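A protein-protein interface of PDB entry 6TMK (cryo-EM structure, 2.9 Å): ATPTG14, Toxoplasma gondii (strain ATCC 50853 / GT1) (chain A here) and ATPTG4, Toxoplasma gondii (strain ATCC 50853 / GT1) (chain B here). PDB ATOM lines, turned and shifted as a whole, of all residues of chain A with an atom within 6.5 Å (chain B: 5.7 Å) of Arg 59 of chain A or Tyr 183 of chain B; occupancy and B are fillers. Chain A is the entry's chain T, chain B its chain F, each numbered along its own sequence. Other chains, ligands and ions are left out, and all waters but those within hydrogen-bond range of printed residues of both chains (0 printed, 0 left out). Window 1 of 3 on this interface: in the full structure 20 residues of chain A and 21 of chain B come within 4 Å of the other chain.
Among the printed residues, pairs that only touch across the chains: Tyr 60 of chain A with Tyr 183 of chain B, Lys 57 of chain A with Leu 82 of chain B, Leu 56 of chain A with Arg 180 of chain B, Gly 58 of chain A with Asp 176 of chain B, Tyr 60 of chain A with Ala 182 of chain B, Arg 59 of chain A with Asp 176 of chain B, Tyr 60 of chain A with Cys 175 of chain B, Gly 58 of chain A with Ala 81 of chain B, Arg 59 of chain A with Pro 179 of chain B, Gly 58 of chain A with Pro 85 of chain B, Arg 59 of chain A with Pro 85 of chain B, Ala 36 of chain A with Ala 81 of chain B and Leu 56 of chain A with Tyr 183 of chain B.
Printed residues of chain B that touch a printed residue of chain A: Ala 80, Ala 81, Leu 82, Ala 83, Pro 85, Cys 175, Asp 176, Pro 179, Arg 180, Ala 182, Tyr 183 and Val 187.
Hydrophobic or aromatic side chains of chain B within 4 Å of the printed part of chain A: Ala 81, Leu 82, Pro 85, Pro 179, Ala 182 and Tyr 183.
Among the printed residues, 20 pairs touch across the chains.
Among the printed residues, no Asp or Glu carboxylate lies within 4 Å of a Lys or Arg side-chain nitrogen of the other chain.
Printed residues of chain B within 4 Å of Gly 58 of chain A: Ala 81 (3.7 Å), Pro 85 (3.8 Å) and Asp 176 (3.6 Å).
Arg 59 of chain A touches just these residues of chain B: Ala 80 (2.9 Å), Ala 81 (2.5 Å), Ala 83 (3.4 Å), Pro 85 (3.8 Å), Asp 176 (3.7 Å), Pro 179 (3.7 Å) and Tyr 183 (3.4 Å).
Printed residues of chain B within 4 Å of Thr 61 of chain A: Tyr 183 (3.2 Å).
Of the printed residues of chain A, Tyr 183 of chain B touches Leu 56, Arg 59, Tyr 60 and Thr 61.
The nearest residue of chain B that does not touch Arg 59 of chain A is Asp 84 of chain B (4.1 Å).
The nearest residue of chain A that does not touch Tyr 183 of chain B is Asn 62 of chain A (5.7 Å).
O of Ala 80 of chain B sits at hydrogen-bond distance from NH1 of Arg 59 of chain A (2.9 Å).
The backbone carbonyl oxygen (O) of Ala 81 of chain B lies within hydrogen-bond range of the guanidinium group (NH1) of Arg 59 of chain A (2.5 Å).
NH1 of Arg 59 of chain A sits at hydrogen-bond distance from O of Ala 83 of chain B (3.4 Å).
The backbone NH (N) of Tyr 60 of chain A lies within hydrogen-bond range of the side-chain carboxylate (OD2) of Asp 176 of chain B, at 3.2 Å.
O of Arg 59 of chain A lies within hydrogen-bond range of OH of Tyr 183 of chain B.
The backbone NH of Thr 61 of chain A sits at hydrogen-bond distance from the side-chain hydroxyl of Tyr 183 of chain B (3.2 Å).
The backbone carbonyl oxygen (O) of Val 187 of chain B sits at hydrogen-bond distance from the side-chain hydroxyl (OH) of Tyr 60 of chain A, 2.6 Å away.
The side-chain carboxylate of Asp 255 of chain B lies within salt-bridge range of the guanidinium group of Arg 180 of chain B, at 3.3 Å.
The backbone carbonyl oxygen (O) of Ala 182 of chain B lies within hydrogen-bond range of the backbone NH (N) of Val 187 of chain B (3.3 Å).
The backbone NH (N) of Arg 59 of chain A lies within hydrogen-bond range of the backbone carbonyl oxygen (O) of Ala 41 of chain A, 2.9 Å away.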
ATOM      1  N   ALA A  36      11.214  10.908 -20.148  1.00  0.00           N
ATOM      2  CA  ALA A  36      12.609  10.508 -20.048  1.00  0.00           C
ATOM      3  C   ALA A  36      13.555  11.444 -20.788  1.00  0.00           C
ATOM      4  O   ALA A  36      14.772  11.253 -20.710  1.00  0.00           O
ATOM      5  CB  ALA A  36      12.777   9.089 -20.588  1.00  0.00           C
ATOM      6  N   ALA A  41      18.211   8.052 -18.283  1.00  0.00           N
ATOM      7  CA  ALA A  41      17.352   6.967 -18.719  1.00  0.00           C
ATOM      8  C   ALA A  41      17.469   5.733 -17.844  1.00  0.00           C
ATOM      9  O   ALA A  41      16.759   4.755 -18.086  1.00  0.00           O
ATOM     10  CB  ALA A  41      17.677   6.594 -20.163  1.00  0.00           C
ATOM     11  N   GLY A  42      18.331   5.754 -16.838  1.00  0.00           N
ATOM     12  CA  GLY A  42      18.557   4.560 -16.050  1.00  0.00           C
ATOM     13  C   GLY A  42      19.083   4.892 -14.676  1.00  0.00           C
ATOM     14  O   GLY A  42      19.481   6.022 -14.383  1.00  0.00           O
ATOM     15  N   LEU A  56      20.393  -2.677 -13.518  1.00  0.00           N
ATOM     16  CA  LEU A  56      20.191  -1.394 -14.175  1.00  0.00           C
ATOM     17  C   LEU A  56      18.723  -1.275 -14.563  1.00  0.00           C
ATOM     18  O   LEU A  56      18.268  -1.936 -15.503  1.00  0.00           O
ATOM     19  CB  LEU A  56      21.095  -1.274 -15.395  1.00  0.00           C
ATOM     20  CG  LEU A  56      21.047   0.039 -16.162  1.00  0.00           C
ATOM     21  CD1 LEU A  56      21.556   1.167 -15.310  1.00  0.00           C
ATOM     22  CD2 LEU A  56      21.871  -0.092 -17.404  1.00  0.00           C
ATOM     23  N   LYS A  57      17.984  -0.441 -13.838  1.00  0.00           N
ATOM     24  CA  LYS A  57      16.584  -0.182 -14.134  1.00  0.00           C
ATOM     25  C   LYS A  57      16.486   0.994 -15.096  1.00  0.00           C
ATOM     26  O   LYS A  57      16.977   2.086 -14.794  1.00  0.00           O
ATOM     27  CB  LYS A  57      15.812   0.116 -12.851  1.00  0.00           C
ATOM     28  CG  LYS A  57      15.993  -0.918 -11.754  1.00  0.00           C
ATOM     29  CD  LYS A  57      15.428  -2.271 -12.139  1.00  0.00           C
ATOM     30  CE  LYS A  57      13.914  -2.256 -12.186  1.00  0.00           C
ATOM     31  NZ  LYS A  57      13.370  -3.627 -12.370  1.00  0.00           N
ATOM     32  N   GLY A  58      15.865   0.774 -16.239  1.00  0.00           N
ATOM     33  CA  GLY A  58      15.574   1.856 -17.153  1.00  0.00           C
ATOM     34  C   GLY A  58      15.667   1.389 -18.594  1.00  0.00           C
ATOM     35  O   GLY A  58      15.411   0.227 -18.900  1.00  0.00           O
ATOM     36  N   ARG A  59      16.034   2.331 -19.452  1.00  0.00           N
ATOM     37  CA  ARG A  59      16.052   2.167 -20.894  1.00  0.00           C
ATOM     38  C   ARG A  59      17.478   2.283 -21.418  1.00  0.00           C
ATOM     39  O   ARG A  59      18.430   2.501 -20.668  1.00  0.00           O
ATOM     40  CB  ARG A  59      15.174   3.224 -21.562  1.00  0.00           C
ATOM     41  CG  ARG A  59      13.711   3.132 -21.264  1.00  0.00           C
ATOM     42  CD  ARG A  59      13.074   4.495 -21.427  1.00  0.00           C
ATOM     43  NE  ARG A  59      11.635   4.413 -21.649  1.00  0.00           N
ATOM     44  CZ  ARG A  59      10.754   4.052 -20.725  1.00  0.00           C
ATOM     45  NH1 ARG A  59      11.155   3.739 -19.503  1.00  0.00           N
ATOM     46  NH2 ARG A  59       9.467   4.011 -21.024  1.00  0.00           N
ATOM     47  N   TYR A  60      17.607   2.133 -22.732  1.00  0.00           N
ATOM     48  CA  TYR A  60      18.840   2.431 -23.437  1.00  0.00           C
ATOM     49  C   TYR A  60      18.901   3.914 -23.774  1.00  0.00           C
ATOM     50  O   TYR A  60      17.876   4.565 -23.983  1.00  0.00           O
ATOM     51  CB  TYR A  60      18.917   1.603 -24.717  1.00  0.00           C
ATOM     52  CG  TYR A  60      20.082   1.915 -25.621  1.00  0.00           C
ATOM     53  CD1 TYR A  60      21.252   1.186 -25.546  1.00  0.00           C
ATOM     54  CD2 TYR A  60      20.006   2.929 -26.558  1.00  0.00           C
ATOM     55  CE1 TYR A  60      22.313   1.462 -26.371  1.00  0.00           C
ATOM     56  CE2 TYR A  60      21.063   3.211 -27.385  1.00  0.00           C
ATOM     57  CZ  TYR A  60      22.217   2.479 -27.285  1.00  0.00           C
ATOM     58  OH  TYR A  60      23.277   2.752 -28.111  1.00  0.00           O
ATOM     59  N   THR A  61      20.118   4.451 -23.827  1.00  0.00           N
ATOM     60  CA  THR A  61      20.299   5.785 -24.374  1.00  0.00           C
ATOM     61  C   THR A  61      21.755   5.987 -24.760  1.00  0.00           C
ATOM     62  O   THR A  61      22.662   5.574 -24.038  1.00  0.00           O
ATOM     63  CB  THR A  61      19.855   6.859 -23.379  1.00  0.00           C
ATOM     64  OG1 THR A  61      19.748   8.119 -24.044  1.00  0.00           O
ATOM     65  CG2 THR A  61      20.836   6.986 -22.256  1.00  0.00           C
ATOM     66  N   ASN A  62      21.958   6.617 -25.914  1.00  0.00           N
ATOM     67  CA  ASN A  62      23.255   7.105 -26.362  1.00  0.00           C
ATOM     68  C   ASN A  62      23.230   8.624 -26.450  1.00  0.00           C
ATOM     69  O   ASN A  62      23.886   9.222 -27.302  1.00  0.00           O
ATOM     70  CB  ASN A  62      23.636   6.489 -27.704  1.00  0.00           C
ATOM     71  CG  ASN A  62      25.127   6.334 -27.870  1.00  0.00           C
ATOM     72  OD1 ASN A  62      25.782   5.632 -27.101  1.00  0.00           O
ATOM     73  ND2 ASN A  62      25.673   6.983 -28.886  1.00  0.00           N
ATOM     74  N   ALA B  80       8.656   7.688 -15.276  1.00  0.00           N
ATOM     75  CA  ALA B  80       8.480   7.332 -16.679  1.00  0.00           C
ATOM     76  C   ALA B  80       9.689   6.575 -17.205  1.00  0.00           C
ATOM     77  O   ALA B  80       9.552   5.528 -17.846  1.00  0.00           O
ATOM     78  CB  ALA B  80       8.236   8.590 -17.504  1.00  0.00           C
ATOM     79  N   ALA B  81      10.888   7.096 -16.946  1.00  0.00           N
ATOM     80  CA  ALA B  81      12.097   6.440 -17.427  1.00  0.00           C
ATOM     81  C   ALA B  81      12.257   5.057 -16.815  1.00  0.00           C
ATOM     82  O   ALA B  81      12.649   4.108 -17.501  1.00  0.00           O
ATOM     83  CB  ALA B  81      13.315   7.304 -17.118  1.00  0.00           C
ATOM     84  N   LEU B  82      11.961   4.923 -15.524  1.00  0.00           N
ATOM     85  CA  LEU B  82      12.101   3.643 -14.848  1.00  0.00           C
ATOM     86  C   LEU B  82      10.933   2.698 -15.093  1.00  0.00           C
ATOM     87  O   LEU B  82      11.006   1.535 -14.686  1.00  0.00           O
ATOM     88  CB  LEU B  82      12.251   3.872 -13.347  1.00  0.00           C
ATOM     89  CG  LEU B  82      13.393   4.789 -12.919  1.00  0.00           C
ATOM     90  CD1 LEU B  82      13.390   4.968 -11.421  1.00  0.00           C
ATOM     91  CD2 LEU B  82      14.726   4.251 -13.385  1.00  0.00           C
ATOM     92  N   ALA B  83       9.866   3.159 -15.740  1.00  0.00           N
ATOM     93  CA  ALA B  83       8.732   2.299 -16.030  1.00  0.00           C
ATOM     94  C   ALA B  83       9.127   1.207 -17.021  1.00  0.00           C
ATOM     95  O   ALA B  83      10.241   1.172 -17.550  1.00  0.00           O
ATOM     96  CB  ALA B  83       7.572   3.127 -16.567  1.00  0.00           C
ATOM     97  N   ASP B  84       8.190   0.305 -17.275  1.00  0.00           N
ATOM     98  CA  ASP B  84       8.416  -0.781 -18.219  1.00  0.00           C
ATOM     99  C   ASP B  84       8.599  -0.215 -19.621  1.00  0.00           C
ATOM    100  O   ASP B  84       7.670   0.409 -20.150  1.00  0.00           O
ATOM    101  CB  ASP B  84       7.249  -1.760 -18.195  1.00  0.00           C
ATOM    102  CG  ASP B  84       7.472  -2.949 -19.106  1.00  0.00           C
ATOM    103  OD1 ASP B  84       6.535  -3.321 -19.842  1.00  0.00           O
ATOM    104  OD2 ASP B  84       8.588  -3.509 -19.091  1.00  0.00           O
ATOM    105  N   PRO B  85       9.760  -0.393 -20.258  1.00  0.00           N
ATOM    106  CA  PRO B  85       9.926   0.135 -21.619  1.00  0.00           C
ATOM    107  C   PRO B  85       9.118  -0.606 -22.666  1.00  0.00           C
ATOM    108  O   PRO B  85       8.869  -0.044 -23.739  1.00  0.00           O
ATOM    109  CB  PRO B  85      11.432  -0.015 -21.877  1.00  0.00           C
ATOM    110  CG  PRO B  85      12.042  -0.260 -20.545  1.00  0.00           C
ATOM    111  CD  PRO B  85      11.012  -0.964 -19.744  1.00  0.00           C
ATOM    112  N   CYS B 175      17.274  -3.789 -26.998  1.00  0.00           N
ATOM    113  CA  CYS B 175      18.133  -2.811 -26.341  1.00  0.00           C
ATOM    114  C   CYS B 175      17.476  -2.225 -25.099  1.00  0.00           C
ATOM    115  O   CYS B 175      18.155  -1.959 -24.102  1.00  0.00           O
ATOM    116  CB  CYS B 175      18.501  -1.709 -27.330  1.00  0.00           C
ATOM    117  SG  CYS B 175      19.696  -2.223 -28.575  1.00  0.00           S
ATOM    118  N   ASP B 176      16.162  -2.008 -25.139  1.00  0.00           N
ATOM    119  CA  ASP B 176      15.481  -1.419 -23.992  1.00  0.00           C
ATOM    120  C   ASP B 176      15.277  -2.428 -22.874  1.00  0.00           C
ATOM    121  O   ASP B 176      15.193  -2.042 -21.704  1.00  0.00           O
ATOM    122  CB  ASP B 176      14.137  -0.836 -24.418  1.00  0.00           C
ATOM    123  CG  ASP B 176      14.263   0.554 -25.010  1.00  0.00           C
ATOM    124  OD1 ASP B 176      13.383   0.944 -25.807  1.00  0.00           O
ATOM    125  OD2 ASP B 176      15.234   1.262 -24.676  1.00  0.00           O
ATOM    126  N   PRO B 179      19.774  -3.148 -21.740  1.00  0.00           N
ATOM    127  CA  PRO B 179      20.675  -2.109 -22.251  1.00  0.00           C
ATOM    128  C   PRO B 179      22.134  -2.400 -21.974  1.00  0.00           C
ATOM    129  O   PRO B 179      22.992  -2.035 -22.785  1.00  0.00           O
ATOM    130  CB  PRO B 179      20.210  -0.846 -21.516  1.00  0.00           C
ATOM    131  CG  PRO B 179      18.945  -1.210 -20.824  1.00  0.00           C
ATOM    132  CD  PRO B 179      18.966  -2.667 -20.617  1.00  0.00           C
ATOM    133  N   ARG B 180      22.443  -3.048 -20.853  1.00  0.00           N
ATOM    134  CA  ARG B 180      23.830  -3.327 -20.517  1.00  0.00           C
ATOM    135  C   ARG B 180      24.491  -4.241 -21.536  1.00  0.00           C
ATOM    136  O   ARG B 180      25.718  -4.213 -21.677  1.00  0.00           O
ATOM    137  CB  ARG B 180      23.903  -3.939 -19.126  1.00  0.00           C
ATOM    138  CG  ARG B 180      23.936  -2.922 -18.020  1.00  0.00           C
ATOM    139  CD  ARG B 180      24.379  -3.548 -16.724  1.00  0.00           C
ATOM    140  NE  ARG B 180      25.809  -3.822 -16.731  1.00  0.00           N
ATOM    141  CZ  ARG B 180      26.400  -4.716 -15.952  1.00  0.00           C
ATOM    142  NH1 ARG B 180      27.703  -4.899 -16.037  1.00  0.00           N
ATOM    143  NH2 ARG B 180      25.692  -5.424 -15.088  1.00  0.00           N
ATOM    144  N   ALA B 181      23.707  -5.052 -22.245  1.00  0.00           N
ATOM    145  CA  ALA B 181      24.249  -5.829 -23.349  1.00  0.00           C
ATOM    146  C   ALA B 181      24.536  -4.953 -24.555  1.00  0.00           C
ATOM    147  O   ALA B 181      25.477  -5.221 -25.309  1.00  0.00           O
ATOM    148  CB  ALA B 181      23.273  -6.937 -23.722  1.00  0.00           C
ATOM    149  N   ALA B 182      23.738  -3.908 -24.751  1.00  0.00           N
ATOM    150  CA  ALA B 182      23.962  -2.997 -25.862  1.00  0.00           C
ATOM    151  C   ALA B 182      25.156  -2.096 -25.596  1.00  0.00           C
ATOM    152  O   ALA B 182      25.937  -1.801 -26.507  1.00  0.00           O
ATOM    153  CB  ALA B 182      22.709  -2.171 -26.108  1.00  0.00           C
ATOM    154  N   TYR B 183      25.314  -1.653 -24.350  1.00  0.00           N
ATOM    155  CA  TYR B 183      26.491  -0.882 -23.981  1.00  0.00           C
ATOM    156  C   TYR B 183      27.751  -1.722 -24.103  1.00  0.00           C
ATOM    157  O   TYR B 183      28.815  -1.215 -24.472  1.00  0.00           O
ATOM    158  CB  TYR B 183      26.342  -0.367 -22.556  1.00  0.00           C
ATOM    159  CG  TYR B 183      25.093   0.436 -22.313  1.00  0.00           C
ATOM    160  CD1 TYR B 183      24.485   1.134 -23.335  1.00  0.00           C
ATOM    161  CD2 TYR B 183      24.528   0.505 -21.055  1.00  0.00           C
ATOM    162  CE1 TYR B 183      23.352   1.869 -23.113  1.00  0.00           C
ATOM    163  CE2 TYR B 183      23.395   1.236 -20.827  1.00  0.00           C
ATOM    164  CZ  TYR B 183      22.812   1.919 -21.860  1.00  0.00           C
ATOM    165  OH  TYR B 183      21.679   2.655 -21.637  1.00  0.00           O
ATOM    166  N   HIS B 184      27.645  -3.011 -23.797  1.00  0.00           N
ATOM    167  CA  HIS B 184      28.790  -3.905 -23.894  1.00  0.00           C
ATOM    168  C   HIS B 184      29.267  -4.036 -25.332  1.00  0.00           C
ATOM    169  O   HIS B 184      30.464  -3.916 -25.616  1.00  0.00           O
ATOM    170  CB  HIS B 184      28.406  -5.268 -23.329  1.00  0.00           C
ATOM    171  CG  HIS B 184      29.509  -6.272 -23.358  1.00  0.00           C
ATOM    172  ND1 HIS B 184      29.931  -6.878 -24.521  1.00  0.00           N
ATOM    173  CD2 HIS B 184      30.258  -6.800 -22.365  1.00  0.00           C
ATOM    174  CE1 HIS B 184      30.906  -7.724 -24.244  1.00  0.00           C
ATOM    175  NE2 HIS B 184      31.124  -7.695 -22.943  1.00  0.00           N
ATOM    176  N   ALA B 185      28.344  -4.288 -26.253  1.00  0.00           N
ATOM    177  CA  ALA B 185      28.682  -4.485 -27.651  1.00  0.00           C
ATOM    178  C   ALA B 185      28.971  -3.189 -28.394  1.00  0.00           C
ATOM    179  O   ALA B 185      29.345  -3.245 -29.569  1.00  0.00           O
ATOM    180  CB  ALA B 185      27.549  -5.229 -28.342  1.00  0.00           C
ATOM    181  N   ARG B 186      28.805  -2.036 -27.752  1.00  0.00           N
ATOM    182  CA  ARG B 186      29.137  -0.753 -28.364  1.00  0.00           C
ATOM    183  C   ARG B 186      28.266  -0.492 -29.585  1.00  0.00           C
ATOM    184  O   ARG B 186      28.738  -0.022 -30.622  1.00  0.00           O
ATOM    185  CB  ARG B 186      30.620  -0.673 -28.731  1.00  0.00           C
ATOM    186  CG  ARG B 186      31.565  -1.053 -27.620  1.00  0.00           C
ATOM    187  CD  ARG B 186      31.436  -0.140 -26.433  1.00  0.00           C
ATOM    188  NE  ARG B 186      31.750   1.249 -26.744  1.00  0.00           N
ATOM    189  CZ  ARG B 186      32.980   1.734 -26.860  1.00  0.00           C
ATOM    190  NH1 ARG B 186      33.156   3.014 -27.139  1.00  0.00           N
ATOM    191  NH2 ARG B 186      34.030   0.946 -26.706  1.00  0.00           N
ATOM    192  N   VAL B 187      26.982  -0.791 -29.461  1.00  0.00           N
ATOM    193  CA  VAL B 187      26.016  -0.517 -30.515  1.00  0.00           C
ATOM    194  C   VAL B 187      25.470   0.889 -30.322  1.00  0.00           C
ATOM    195  O   VAL B 187      25.072   1.267 -29.214  1.00  0.00           O
ATOM    196  CB  VAL B 187      24.882  -1.554 -30.511  1.00  0.00           C
ATOM    197  CG1 VAL B 187      25.438  -2.951 -30.497  1.00  0.00           C
ATOM    198  CG2 VAL B 187      23.974  -1.343 -29.347  1.00  0.00           C
ATOM    199  N   VAL B 254      33.651   1.278 -20.331  1.00  0.00           N
ATOM    200  CA  VAL B 254      32.423   1.237 -21.108  1.00  0.00           C
ATOM    201  C   VAL B 254      31.213   1.251 -20.188  1.00  0.00           C
ATOM    202  O   VAL B 254      30.257   2.003 -20.402  1.00  0.00           O
ATOM    203  CB  VAL B 254      32.428  -0.008 -22.010  1.00  0.00           C
ATOM    204  CG1 VAL B 254      31.093  -0.195 -22.674  1.00  0.00           C
ATOM    205  CG2 VAL B 254      33.531   0.090 -23.026  1.00  0.00           C
ATOM    206  N   ASP B 255      31.246   0.426 -19.149  1.00  0.00           N
ATOM    207  CA  ASP B 255      30.166   0.326 -18.175  1.00  0.00           C
ATOM    208  C   ASP B 255      30.802   0.158 -16.804  1.00  0.00           C
ATOM    209  O   ASP B 255      31.317  -0.917 -16.486  1.00  0.00           O
ATOM    210  CB  ASP B 255      29.244  -0.846 -18.497  1.00  0.00           C
ATOM    211  CG  ASP B 255      27.903  -0.740 -17.810  1.00  0.00           C
ATOM    212  OD1 ASP B 255      26.957  -0.216 -18.432  1.00  0.00           O
ATOM    213  OD2 ASP B 255      27.789  -1.179 -16.650  1.00  0.00           O
